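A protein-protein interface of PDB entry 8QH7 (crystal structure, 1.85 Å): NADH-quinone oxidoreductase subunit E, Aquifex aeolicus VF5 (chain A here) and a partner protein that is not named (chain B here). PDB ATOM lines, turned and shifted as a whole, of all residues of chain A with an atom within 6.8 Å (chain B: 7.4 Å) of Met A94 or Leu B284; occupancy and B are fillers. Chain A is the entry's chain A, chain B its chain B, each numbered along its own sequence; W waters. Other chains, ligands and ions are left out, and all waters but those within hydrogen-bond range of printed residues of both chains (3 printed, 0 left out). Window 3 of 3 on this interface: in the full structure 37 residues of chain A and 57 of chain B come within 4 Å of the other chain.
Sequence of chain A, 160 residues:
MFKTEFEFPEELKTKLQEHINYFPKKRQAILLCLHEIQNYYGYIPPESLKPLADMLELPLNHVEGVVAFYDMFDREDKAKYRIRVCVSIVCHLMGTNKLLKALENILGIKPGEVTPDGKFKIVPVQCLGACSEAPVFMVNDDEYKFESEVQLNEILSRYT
The backbone carbonyl oxygen (O) of Lys B257 is in hydrogen-bond range of the backbone NH (N) of Leu B284, 3.0 Å away.
N of Lys B257 sits at hydrogen-bond distance from O of Val B324 (3.0 Å).
N of Val B324 is in hydrogen-bond range of O of Ser B255.
The backbone NH of Thr B326 sits at hydrogen-bond distance from the side-chain carboxylate of Asp B329 (2.9 Å).
NZ of Lys B257 lies within salt-bridge range of OD1 of Asp B329, 2.7 Å away.
Ser B255 touches Val A90.
CG1 of Val A90 touches N of Gly B256 (3.8 Å).
CD2 of Leu A93 touches OD1 of Asp B329, 3.9 Å away.
O of Gly B256 touches SD of Met A94, 3.99 Å away.
SD of Met A94 touches CE of Lys B257, at 3.8 Å.
CE of Met A94 touches CD1 of Leu B284, at 3.97 Å.
Cys A131 touches Ser B255.
Of the printed residues of chain B, Met A94 touches Gly B256, Lys B257 and Leu B284.
Of chain A, only Met A94 (3.97 Å) comes within 4 Å of Leu B284.
Printed residues of chain A within 4 Å of Asp B329: Leu A93 (3.9 Å).
Of the printed residues of chain A, Lys B257 touches Met A94.
Of the printed residues of chain B, Val A90 touches Ser B255 and Gly B256.
Gly B282 touches none of the printed residues of chain A.
The nearest printed residue of chain B that does not touch Met A94 is Val B258 (6.2 Å).
The nearest printed residue of chain A that does not touch Leu B284 is Leu A93 (7.8 Å).
The nearest printed residue of chain A that does not touch Lys B257 is Leu A93 (4.01 Å).
Printed residues of chain B that touch a printed residue of chain A: Ser B255, Gly B256, Lys B257, Leu B284 and Asp B329.
Of the 15 printed residues of chain A, 4 touch a printed residue of chain B.
Hydrophobic or aromatic side chains of chain A within 4 Å of the printed part of chain B: Val A90, Leu A93 and Met A94.
Along chain A the printed residues that touch a printed residue of chain B span positions 90 to 131.
Among the printed residues, no Asp or Glu carboxylate lies within 4 Å of a Lys or Arg side-chain nitrogen of the other chain.
Water W1 bridges the side-chain carboxylate of Glu A133 and the backbone carbonyl oxygen of Pro B261.
Water W3 lies within hydrogen-bond range of the backbone carbonyl oxygen of Leu A93 (2.7 Å) and the side-chain amino group of Lys B257 (3.2 Å).
Water W2 lies within hydrogen-bond range of the backbone carbonyl oxygen of Cys A131 (2.7 Å) and the backbone NH of Gly B256 (2.9 Å).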
ATOM      1  N   ILE A  89     -21.987   4.536  11.442  1.00  0.00           N
ATOM      2  CA  ILE A  89     -21.774   5.653  12.362  1.00  0.00           C
ATOM      3  C   ILE A  89     -20.289   6.024  12.504  1.00  0.00           C
ATOM      4  O   ILE A  89     -19.949   7.198  12.354  1.00  0.00           O
ATOM      5  CB  ILE A  89     -22.478   5.399  13.717  1.00  0.00           C
ATOM      6  CG1 ILE A  89     -22.219   6.496  14.754  1.00  0.00           C
ATOM      7  CG2 ILE A  89     -22.168   4.027  14.291  1.00  0.00           C
ATOM      8  CD1 ILE A  89     -22.854   7.799  14.428  1.00  0.00           C
ATOM      9  N   VAL A  90     -19.387   5.084  12.812  1.00  0.00           N
ATOM     10  CA  VAL A  90     -18.016   5.482  13.132  1.00  0.00           C
ATOM     11  C   VAL A  90     -17.313   6.035  11.890  1.00  0.00           C
ATOM     12  O   VAL A  90     -16.696   7.099  11.945  1.00  0.00           O
ATOM     13  CB  VAL A  90     -17.195   4.350  13.774  1.00  0.00           C
ATOM     14  CG1 VAL A  90     -15.887   4.884  14.353  1.00  0.00           C
ATOM     15  CG2 VAL A  90     -17.989   3.614  14.846  1.00  0.00           C
ATOM     16  N   CYS A  91     -17.396   5.320  10.766  1.00  0.00           N
ATOM     17  CA  CYS A  91     -16.759   5.788   9.546  1.00  0.00           C
ATOM     18  C   CYS A  91     -17.354   7.128   9.114  1.00  0.00           C
ATOM     19  O   CYS A  91     -16.616   7.986   8.640  1.00  0.00           O
ATOM     20  CB  CYS A  91     -16.825   4.727   8.458  1.00  0.00           C
ATOM     21  SG  CYS A  91     -15.825   3.270   8.879  1.00  0.00           S
ATOM     22  N   HIS A  92     -18.668   7.316   9.318  1.00  0.00           N
ATOM     23  CA  HIS A  92     -19.300   8.587   9.007  1.00  0.00           C
ATOM     24  C   HIS A  92     -18.659   9.712   9.824  1.00  0.00           C
ATOM     25  O   HIS A  92     -18.312  10.748   9.262  1.00  0.00           O
ATOM     26  CB  HIS A  92     -20.816   8.545   9.216  1.00  0.00           C
ATOM     27  CG  HIS A  92     -21.405   9.888   8.928  1.00  0.00           C
ATOM     28  ND1 HIS A  92     -21.598  10.372   7.650  1.00  0.00           N
ATOM     29  CD2 HIS A  92     -21.778  10.852   9.764  1.00  0.00           C
ATOM     30  CE1 HIS A  92     -22.109  11.590   7.730  1.00  0.00           C
ATOM     31  NE2 HIS A  92     -22.224  11.901   9.011  1.00  0.00           N
ATOM     32  N   LEU A  93     -18.512   9.491  11.138  1.00  0.00           N
ATOM     33  CA  LEU A  93     -17.863  10.435  12.044  1.00  0.00           C
ATOM     34  C   LEU A  93     -16.427  10.751  11.622  1.00  0.00           C
ATOM     35  O   LEU A  93     -15.986  11.876  11.818  1.00  0.00           O
ATOM     36  CB  LEU A  93     -17.833   9.860  13.465  1.00  0.00           C
ATOM     37  CG  LEU A  93     -19.142   9.912  14.253  1.00  0.00           C
ATOM     38  CD1 LEU A  93     -18.966   9.196  15.582  1.00  0.00           C
ATOM     39  CD2 LEU A  93     -19.598  11.346  14.470  1.00  0.00           C
ATOM     40  N   MET A  94     -15.693   9.753  11.105  1.00  0.00           N
ATOM     41  CA  MET A  94     -14.252   9.866  10.924  1.00  0.00           C
ATOM     42  C   MET A  94     -13.843  10.127   9.469  1.00  0.00           C
ATOM     43  O   MET A  94     -12.649  10.302   9.217  1.00  0.00           O
ATOM     44  CB  MET A  94     -13.557   8.590  11.411  1.00  0.00           C
ATOM     45  CG  MET A  94     -13.872   8.234  12.856  1.00  0.00           C
ATOM     46  SD  MET A  94     -13.548   9.572  14.018  1.00  0.00           S
ATOM     47  CE  MET A  94     -11.775   9.765  13.842  1.00  0.00           C
ATOM     48  N   GLY A  95     -14.786  10.129   8.508  1.00  0.00           N
ATOM     49  CA  GLY A  95     -14.506  10.675   7.181  1.00  0.00           C
ATOM     50  C   GLY A  95     -14.954   9.835   5.975  1.00  0.00           C
ATOM     51  O   GLY A  95     -14.321   9.905   4.920  1.00  0.00           O
ATOM     52  N   THR A  96     -16.082   9.119   6.069  1.00  0.00           N
ATOM     53  CA  THR A  96     -16.652   8.430   4.918  1.00  0.00           C
ATOM     54  C   THR A  96     -16.776   9.369   3.715  1.00  0.00           C
ATOM     55  O   THR A  96     -16.467   8.970   2.594  1.00  0.00           O
ATOM     56  CB  THR A  96     -18.039   7.843   5.221  1.00  0.00           C
ATOM     57  OG1 THR A  96     -17.872   6.833   6.210  1.00  0.00           O
ATOM     58  CG2 THR A  96     -18.739   7.249   4.015  1.00  0.00           C
ATOM     59  N   ASN A  97     -17.243  10.608   3.932  1.00  0.00           N
ATOM     60  CA  ASN A  97     -17.508  11.508   2.814  1.00  0.00           C
ATOM     61  C   ASN A  97     -16.201  11.918   2.125  1.00  0.00           C
ATOM     62  O   ASN A  97     -16.188  12.160   0.920  1.00  0.00           O
ATOM     63  CB  ASN A  97     -18.381  12.696   3.234  1.00  0.00           C
ATOM     64  CG  ASN A  97     -19.809  12.297   3.578  1.00  0.00           C
ATOM     65  OD1 ASN A  97     -20.546  13.095   4.148  1.00  0.00           O
ATOM     66  ND2 ASN A  97     -20.224  11.076   3.268  1.00  0.00           N
ATOM     67  N   LYS A  98     -15.098  11.976   2.876  1.00  0.00           N
ATOM     68  CA  LYS A  98     -13.791  12.295   2.305  1.00  0.00           C
ATOM     69  C   LYS A  98     -13.327  11.165   1.388  1.00  0.00           C
ATOM     70  O   LYS A  98     -12.864  11.412   0.276  1.00  0.00           O
ATOM     71  CB  LYS A  98     -12.772  12.558   3.416  1.00  0.00           C
ATOM     72  CG  LYS A  98     -13.134  13.737   4.307  1.00  0.00           C
ATOM     73  CD  LYS A  98     -12.121  14.042   5.385  1.00  0.00           C
ATOM     74  CE  LYS A  98     -12.359  15.394   6.027  1.00  0.00           C
ATOM     75  NZ  LYS A  98     -11.478  15.596   7.202  1.00  0.00           N
ATOM     76  N   CYS A 131     -13.726  -0.435  13.032  1.00  0.00           N
ATOM     77  CA  CYS A 131     -14.141   0.940  13.259  1.00  0.00           C
ATOM     78  C   CYS A 131     -12.999   1.800  13.812  1.00  0.00           C
ATOM     79  O   CYS A 131     -12.999   3.017  13.622  1.00  0.00           O
ATOM     80  CB  CYS A 131     -15.341   0.968  14.201  1.00  0.00           C
ATOM     81  SG  CYS A 131     -16.565  -0.326  13.855  1.00  0.00           S
ATOM     82  N   GLU A 133     -10.155   1.858  12.688  1.00  0.00           N
ATOM     83  CA  GLU A 133      -9.374   2.197  11.508  1.00  0.00           C
ATOM     84  C   GLU A 133     -10.263   2.937  10.501  1.00  0.00           C
ATOM     85  O   GLU A 133     -10.005   2.950   9.298  1.00  0.00           O
ATOM     86  CB  GLU A 133      -8.740   0.890  11.019  1.00  0.00           C
ATOM     87  CG  GLU A 133      -7.738   0.314  12.028  1.00  0.00           C
ATOM     88  CD  GLU A 133      -6.522   1.182  12.268  1.00  0.00           C
ATOM     89  OE1 GLU A 133      -6.223   1.490  13.449  1.00  0.00           O
ATOM     90  OE2 GLU A 133      -5.873   1.575  11.277  1.00  0.00           O
ATOM     91  N   ALA A 134     -11.302   3.605  11.017  1.00  0.00           N
ATOM     92  CA  ALA A 134     -12.225   4.368  10.191  1.00  0.00           C
ATOM     93  C   ALA A 134     -11.512   5.545   9.536  1.00  0.00           C
ATOM     94  O   ALA A 134     -10.595   6.122  10.131  1.00  0.00           O
ATOM     95  CB  ALA A 134     -13.371   4.866  11.035  1.00  0.00           C
ATOM     96  N   PRO A 135     -11.920   5.970   8.317  1.00  0.00           N
ATOM     97  CA  PRO A 135     -12.954   5.290   7.524  1.00  0.00           C
ATOM     98  C   PRO A 135     -12.448   4.081   6.735  1.00  0.00           C
ATOM     99  O   PRO A 135     -11.381   4.138   6.138  1.00  0.00           O
ATOM    100  CB  PRO A 135     -13.462   6.392   6.582  1.00  0.00           C
ATOM    101  CG  PRO A 135     -12.308   7.339   6.429  1.00  0.00           C
ATOM    102  CD  PRO A 135     -11.472   7.220   7.688  1.00  0.00           C
ATOM    103  N   PHE A 146      -8.772   4.288   4.928  1.00  0.00           N
ATOM    104  CA  PHE A 146      -8.514   5.431   4.064  1.00  0.00           C
ATOM    105  C   PHE A 146      -7.728   6.490   4.832  1.00  0.00           C
ATOM    106  O   PHE A 146      -8.157   6.904   5.907  1.00  0.00           O
ATOM    107  CB  PHE A 146      -9.828   6.047   3.561  1.00  0.00           C
ATOM    108  CG  PHE A 146      -9.669   7.359   2.833  1.00  0.00           C
ATOM    109  CD1 PHE A 146      -9.226   7.400   1.520  1.00  0.00           C
ATOM    110  CD2 PHE A 146      -9.992   8.561   3.452  1.00  0.00           C
ATOM    111  CE1 PHE A 146      -9.111   8.606   0.844  1.00  0.00           C
ATOM    112  CE2 PHE A 146      -9.860   9.769   2.779  1.00  0.00           C
ATOM    113  CZ  PHE A 146      -9.419   9.790   1.475  1.00  0.00           C
ATOM    114  N   SER B 255     -13.632   3.131  19.660  1.00  0.00           N
ATOM    115  CA  SER B 255     -13.495   3.868  18.410  1.00  0.00           C
ATOM    116  C   SER B 255     -14.080   5.280  18.533  1.00  0.00           C
ATOM    117  O   SER B 255     -14.590   5.675  19.585  1.00  0.00           O
ATOM    118  CB  SER B 255     -14.131   3.098  17.279  1.00  0.00           C
ATOM    119  OG  SER B 255     -15.533   2.927  17.480  1.00  0.00           O
ATOM    120  N   GLY B 256     -14.024   6.027  17.423  1.00  0.00           N
ATOM    121  CA  GLY B 256     -14.493   7.398  17.402  1.00  0.00           C
ATOM    122  C   GLY B 256     -13.385   8.339  17.852  1.00  0.00           C
ATOM    123  O   GLY B 256     -12.221   8.133  17.498  1.00  0.00           O
ATOM    124  N   LYS B 257     -13.749   9.322  18.682  1.00  0.00           N
ATOM    125  CA  LYS B 257     -12.895  10.464  18.935  1.00  0.00           C
ATOM    126  C   LYS B 257     -11.971  10.203  20.124  1.00  0.00           C
ATOM    127  O   LYS B 257     -11.943  11.004  21.054  1.00  0.00           O
ATOM    128  CB  LYS B 257     -13.752  11.708  19.179  1.00  0.00           C
ATOM    129  CG  LYS B 257     -14.741  12.013  18.065  1.00  0.00           C
ATOM    130  CD  LYS B 257     -14.068  12.265  16.728  1.00  0.00           C
ATOM    131  CE  LYS B 257     -15.072  12.616  15.649  1.00  0.00           C
ATOM    132  NZ  LYS B 257     -15.629  13.972  15.853  1.00  0.00           N
ATOM    133  N   VAL B 258     -11.220   9.093  20.072  1.00  0.00           N
ATOM    134  CA  VAL B 258     -10.181   8.818  21.050  1.00  0.00           C
ATOM    135  C   VAL B 258      -8.818   8.840  20.358  1.00  0.00           C
ATOM    136  O   VAL B 258      -8.715   8.609  19.154  1.00  0.00           O
ATOM    137  CB  VAL B 258     -10.423   7.488  21.787  1.00  0.00           C
ATOM    138  CG1 VAL B 258     -11.725   7.538  22.574  1.00  0.00           C
ATOM    139  CG2 VAL B 258     -10.402   6.297  20.837  1.00  0.00           C
ATOM    140  N   LYS B 259      -7.767   9.079  21.149  1.00  0.00           N
ATOM    141  CA  LYS B 259      -6.416   9.143  20.617  1.00  0.00           C
ATOM    142  C   LYS B 259      -5.909   7.757  20.226  1.00  0.00           C
ATOM    143  O   LYS B 259      -5.174   7.648  19.253  1.00  0.00           O
ATOM    144  CB  LYS B 259      -5.446   9.792  21.612  1.00  0.00           C
ATOM    145  CG  LYS B 259      -5.723  11.250  21.939  1.00  0.00           C
ATOM    146  CD  LYS B 259      -4.508  11.935  22.567  1.00  0.00           C
ATOM    147  CE  LYS B 259      -4.784  13.317  23.125  1.00  0.00           C
ATOM    148  NZ  LYS B 259      -5.850  13.293  24.159  1.00  0.00           N
ATOM    149  N   LYS B 260      -6.314   6.704  20.949  1.00  0.00           N
ATOM    150  CA  LYS B 260      -5.790   5.363  20.724  1.00  0.00           C
ATOM    151  C   LYS B 260      -6.932   4.374  20.485  1.00  0.00           C
ATOM    152  O   LYS B 260      -7.130   3.440  21.262  1.00  0.00           O
ATOM    153  CB  LYS B 260      -4.962   4.877  21.919  1.00  0.00           C
ATOM    154  CG  LYS B 260      -3.719   5.689  22.267  1.00  0.00           C
ATOM    155  CD  LYS B 260      -3.103   5.304  23.615  1.00  0.00           C
ATOM    156  CE  LYS B 260      -3.021   3.801  23.843  1.00  0.00           C
ATOM    157  NZ  LYS B 260      -2.562   3.462  25.214  1.00  0.00           N
ATOM    158  N   PRO B 261      -7.678   4.490  19.362  1.00  0.00           N
ATOM    159  CA  PRO B 261      -8.777   3.566  19.092  1.00  0.00           C
ATOM    160  C   PRO B 261      -8.180   2.177  18.889  1.00  0.00           C
ATOM    161  O   PRO B 261      -7.061   2.046  18.378  1.00  0.00           O
ATOM    162  CB  PRO B 261      -9.437   4.158  17.836  1.00  0.00           C
ATOM    163  CG  PRO B 261      -8.319   4.895  17.136  1.00  0.00           C
ATOM    164  CD  PRO B 261      -7.442   5.429  18.252  1.00  0.00           C
ATOM    165  N   ALA B 280      -7.455   4.494  26.479  1.00  0.00           N
ATOM    166  CA  ALA B 280      -7.549   4.860  25.068  1.00  0.00           C
ATOM    167  C   ALA B 280      -6.935   6.241  24.797  1.00  0.00           C
ATOM    168  O   ALA B 280      -7.037   6.749  23.684  1.00  0.00           O
ATOM    169  CB  ALA B 280      -8.985   4.795  24.600  1.00  0.00           C
ATOM    170  N   GLY B 281      -6.314   6.848  25.813  1.00  0.00           N
ATOM    171  CA  GLY B 281      -5.475   8.030  25.640  1.00  0.00           C
ATOM    172  C   GLY B 281      -6.238   9.352  25.673  1.00  0.00           C
ATOM    173  O   GLY B 281      -5.665  10.409  25.384  1.00  0.00           O
ATOM    174  N   GLY B 282      -7.517   9.313  26.060  1.00  0.00           N
ATOM    175  CA  GLY B 282      -8.323  10.522  26.103  1.00  0.00           C
ATOM    176  C   GLY B 282      -8.914  10.828  24.733  1.00  0.00           C
ATOM    177  O   GLY B 282      -8.869   9.992  23.839  1.00  0.00           O
ATOM    178  N   THR B 283      -9.453  12.038  24.577  1.00  0.00           N
ATOM    179  CA  THR B 283     -10.195  12.382  23.372  1.00  0.00           C
ATOM    180  C   THR B 283      -9.272  13.048  22.354  1.00  0.00           C
ATOM    181  O   THR B 283      -8.268  13.655  22.721  1.00  0.00           O
ATOM    182  CB  THR B 283     -11.393  13.281  23.699  1.00  0.00           C
ATOM    183  OG1 THR B 283     -10.892  14.451  24.334  1.00  0.00           O
ATOM    184  CG2 THR B 283     -12.425  12.607  24.579  1.00  0.00           C
ATOM    185  N   LEU B 284      -9.617  12.908  21.067  1.00  0.00           N
ATOM    186  CA  LEU B 284      -8.981  13.678  20.012  1.00  0.00           C
ATOM    187  C   LEU B 284      -9.141  15.164  20.317  1.00  0.00           C
ATOM    188  O   LEU B 284     -10.248  15.630  20.587  1.00  0.00           O
ATOM    189  CB  LEU B 284      -9.615  13.346  18.657  1.00  0.00           C
ATOM    190  CG  LEU B 284      -9.159  12.028  18.034  1.00  0.00           C
ATOM    191  CD1 LEU B 284      -9.950  11.723  16.772  1.00  0.00           C
ATOM    192  CD2 LEU B 284      -7.660  12.059  17.733  1.00  0.00           C
ATOM    193  N   GLY B 285      -8.012  15.879  20.306  1.00  0.00           N
ATOM    194  CA  GLY B 285      -7.970  17.314  20.551  1.00  0.00           C
ATOM    195  C   GLY B 285      -8.320  17.685  21.993  1.00  0.00           C
ATOM    196  O   GLY B 285      -8.547  18.850  22.286  1.00  0.00           O
ATOM    197  N   ASN B 286      -8.401  16.683  22.882  1.00  0.00           N
ATOM    198  CA  ASN B 286      -8.818  16.898  24.260  1.00  0.00           C
ATOM    199  C   ASN B 286     -10.159  17.635  24.311  1.00  0.00           C
ATOM    200  O   ASN B 286     -10.395  18.431  25.212  1.00  0.00           O
ATOM    201  CB  ASN B 286      -7.735  17.619  25.067  1.00  0.00           C
ATOM    202  CG  ASN B 286      -6.437  16.841  25.100  1.00  0.00           C
ATOM    203  OD1 ASN B 286      -6.442  15.637  25.336  1.00  0.00           O
ATOM    204  ND2 ASN B 286      -5.320  17.512  24.868  1.00  0.00           N
ATOM    205  N   LYS B 287     -11.042  17.363  23.345  1.00  0.00           N
ATOM    206  CA  LYS B 287     -12.408  17.859  23.411  1.00  0.00           C
ATOM    207  C   LYS B 287     -13.161  17.094  24.498  1.00  0.00           C
ATOM    208  O   LYS B 287     -12.768  15.997  24.895  1.00  0.00           O
ATOM    209  CB  LYS B 287     -13.155  17.682  22.083  1.00  0.00           C
ATOM    210  CG  LYS B 287     -12.522  18.308  20.849  1.00  0.00           C
ATOM    211  CD  LYS B 287     -12.110  19.758  21.016  1.00  0.00           C
ATOM    212  CE  LYS B 287     -12.302  20.591  19.763  1.00  0.00           C
ATOM    213  NZ  LYS B 287     -11.942  19.857  18.521  1.00  0.00           N
ATOM    214  N   LYS B 288     -14.272  17.679  24.947  1.00  0.00           N
ATOM    215  CA  LYS B 288     -15.096  17.075  25.975  1.00  0.00           C
ATOM    216  C   LYS B 288     -15.911  15.943  25.367  1.00  0.00           C
ATOM    217  O   LYS B 288     -16.418  16.061  24.248  1.00  0.00           O
ATOM    218  CB  LYS B 288     -16.026  18.119  26.599  1.00  0.00           C
ATOM    219  CG  LYS B 288     -15.292  19.176  27.400  1.00  0.00           C
ATOM    220  CD  LYS B 288     -16.143  20.352  27.794  1.00  0.00           C
ATOM    221  CE  LYS B 288     -16.684  20.276  29.205  1.00  0.00           C
ATOM    222  NZ  LYS B 288     -16.820  21.636  29.785  1.00  0.00           N
ATOM    223  N   VAL B 324     -16.956   6.853  20.914  1.00  0.00           N
ATOM    224  CA  VAL B 324     -16.891   8.126  21.610  1.00  0.00           C
ATOM    225  C   VAL B 324     -17.225   9.250  20.633  1.00  0.00           C
ATOM    226  O   VAL B 324     -16.606   9.357  19.576  1.00  0.00           O
ATOM    227  CB  VAL B 324     -15.513   8.347  22.263  1.00  0.00           C
ATOM    228  CG1 VAL B 324     -15.446   9.689  22.958  1.00  0.00           C
ATOM    229  CG2 VAL B 324     -15.148   7.221  23.221  1.00  0.00           C
ATOM    230  N   THR B 326     -17.593  13.555  20.667  1.00  0.00           N
ATOM    231  CA  THR B 326     -17.184  14.708  21.451  1.00  0.00           C
ATOM    232  C   THR B 326     -18.101  15.895  21.167  1.00  0.00           C
ATOM    233  O   THR B 326     -19.039  15.805  20.372  1.00  0.00           O
ATOM    234  CB  THR B 326     -15.690  14.997  21.253  1.00  0.00           C
ATOM    235  OG1 THR B 326     -15.469  15.085  19.849  1.00  0.00           O
ATOM    236  CG2 THR B 326     -14.816  13.928  21.871  1.00  0.00           C
ATOM    237  N   ASP B 329     -19.802  16.851  17.848  1.00  0.00           N
ATOM    238  CA  ASP B 329     -20.524  15.875  17.043  1.00  0.00           C
ATOM    239  C   ASP B 329     -22.023  16.076  17.244  1.00  0.00           C
ATOM    240  O   ASP B 329     -22.504  16.098  18.376  1.00  0.00           O
ATOM    241  CB  ASP B 329     -20.090  14.439  17.356  1.00  0.00           C
ATOM    242  CG  ASP B 329     -18.631  14.191  17.004  1.00  0.00           C
ATOM    243  OD1 ASP B 329     -18.214  14.694  15.938  1.00  0.00           O
ATOM    244  OD2 ASP B 329     -17.918  13.506  17.790  1.00  0.00           O
HETATM  245  O   HOH W   1      -6.404   0.755  15.825  1.00  0.00           O
HETATM  246  O   HOH W   2     -12.447   5.197  15.114  1.00  0.00           O
HETATM  247  O   HOH W   3     -16.587  14.264  12.855  1.00  0.00           O
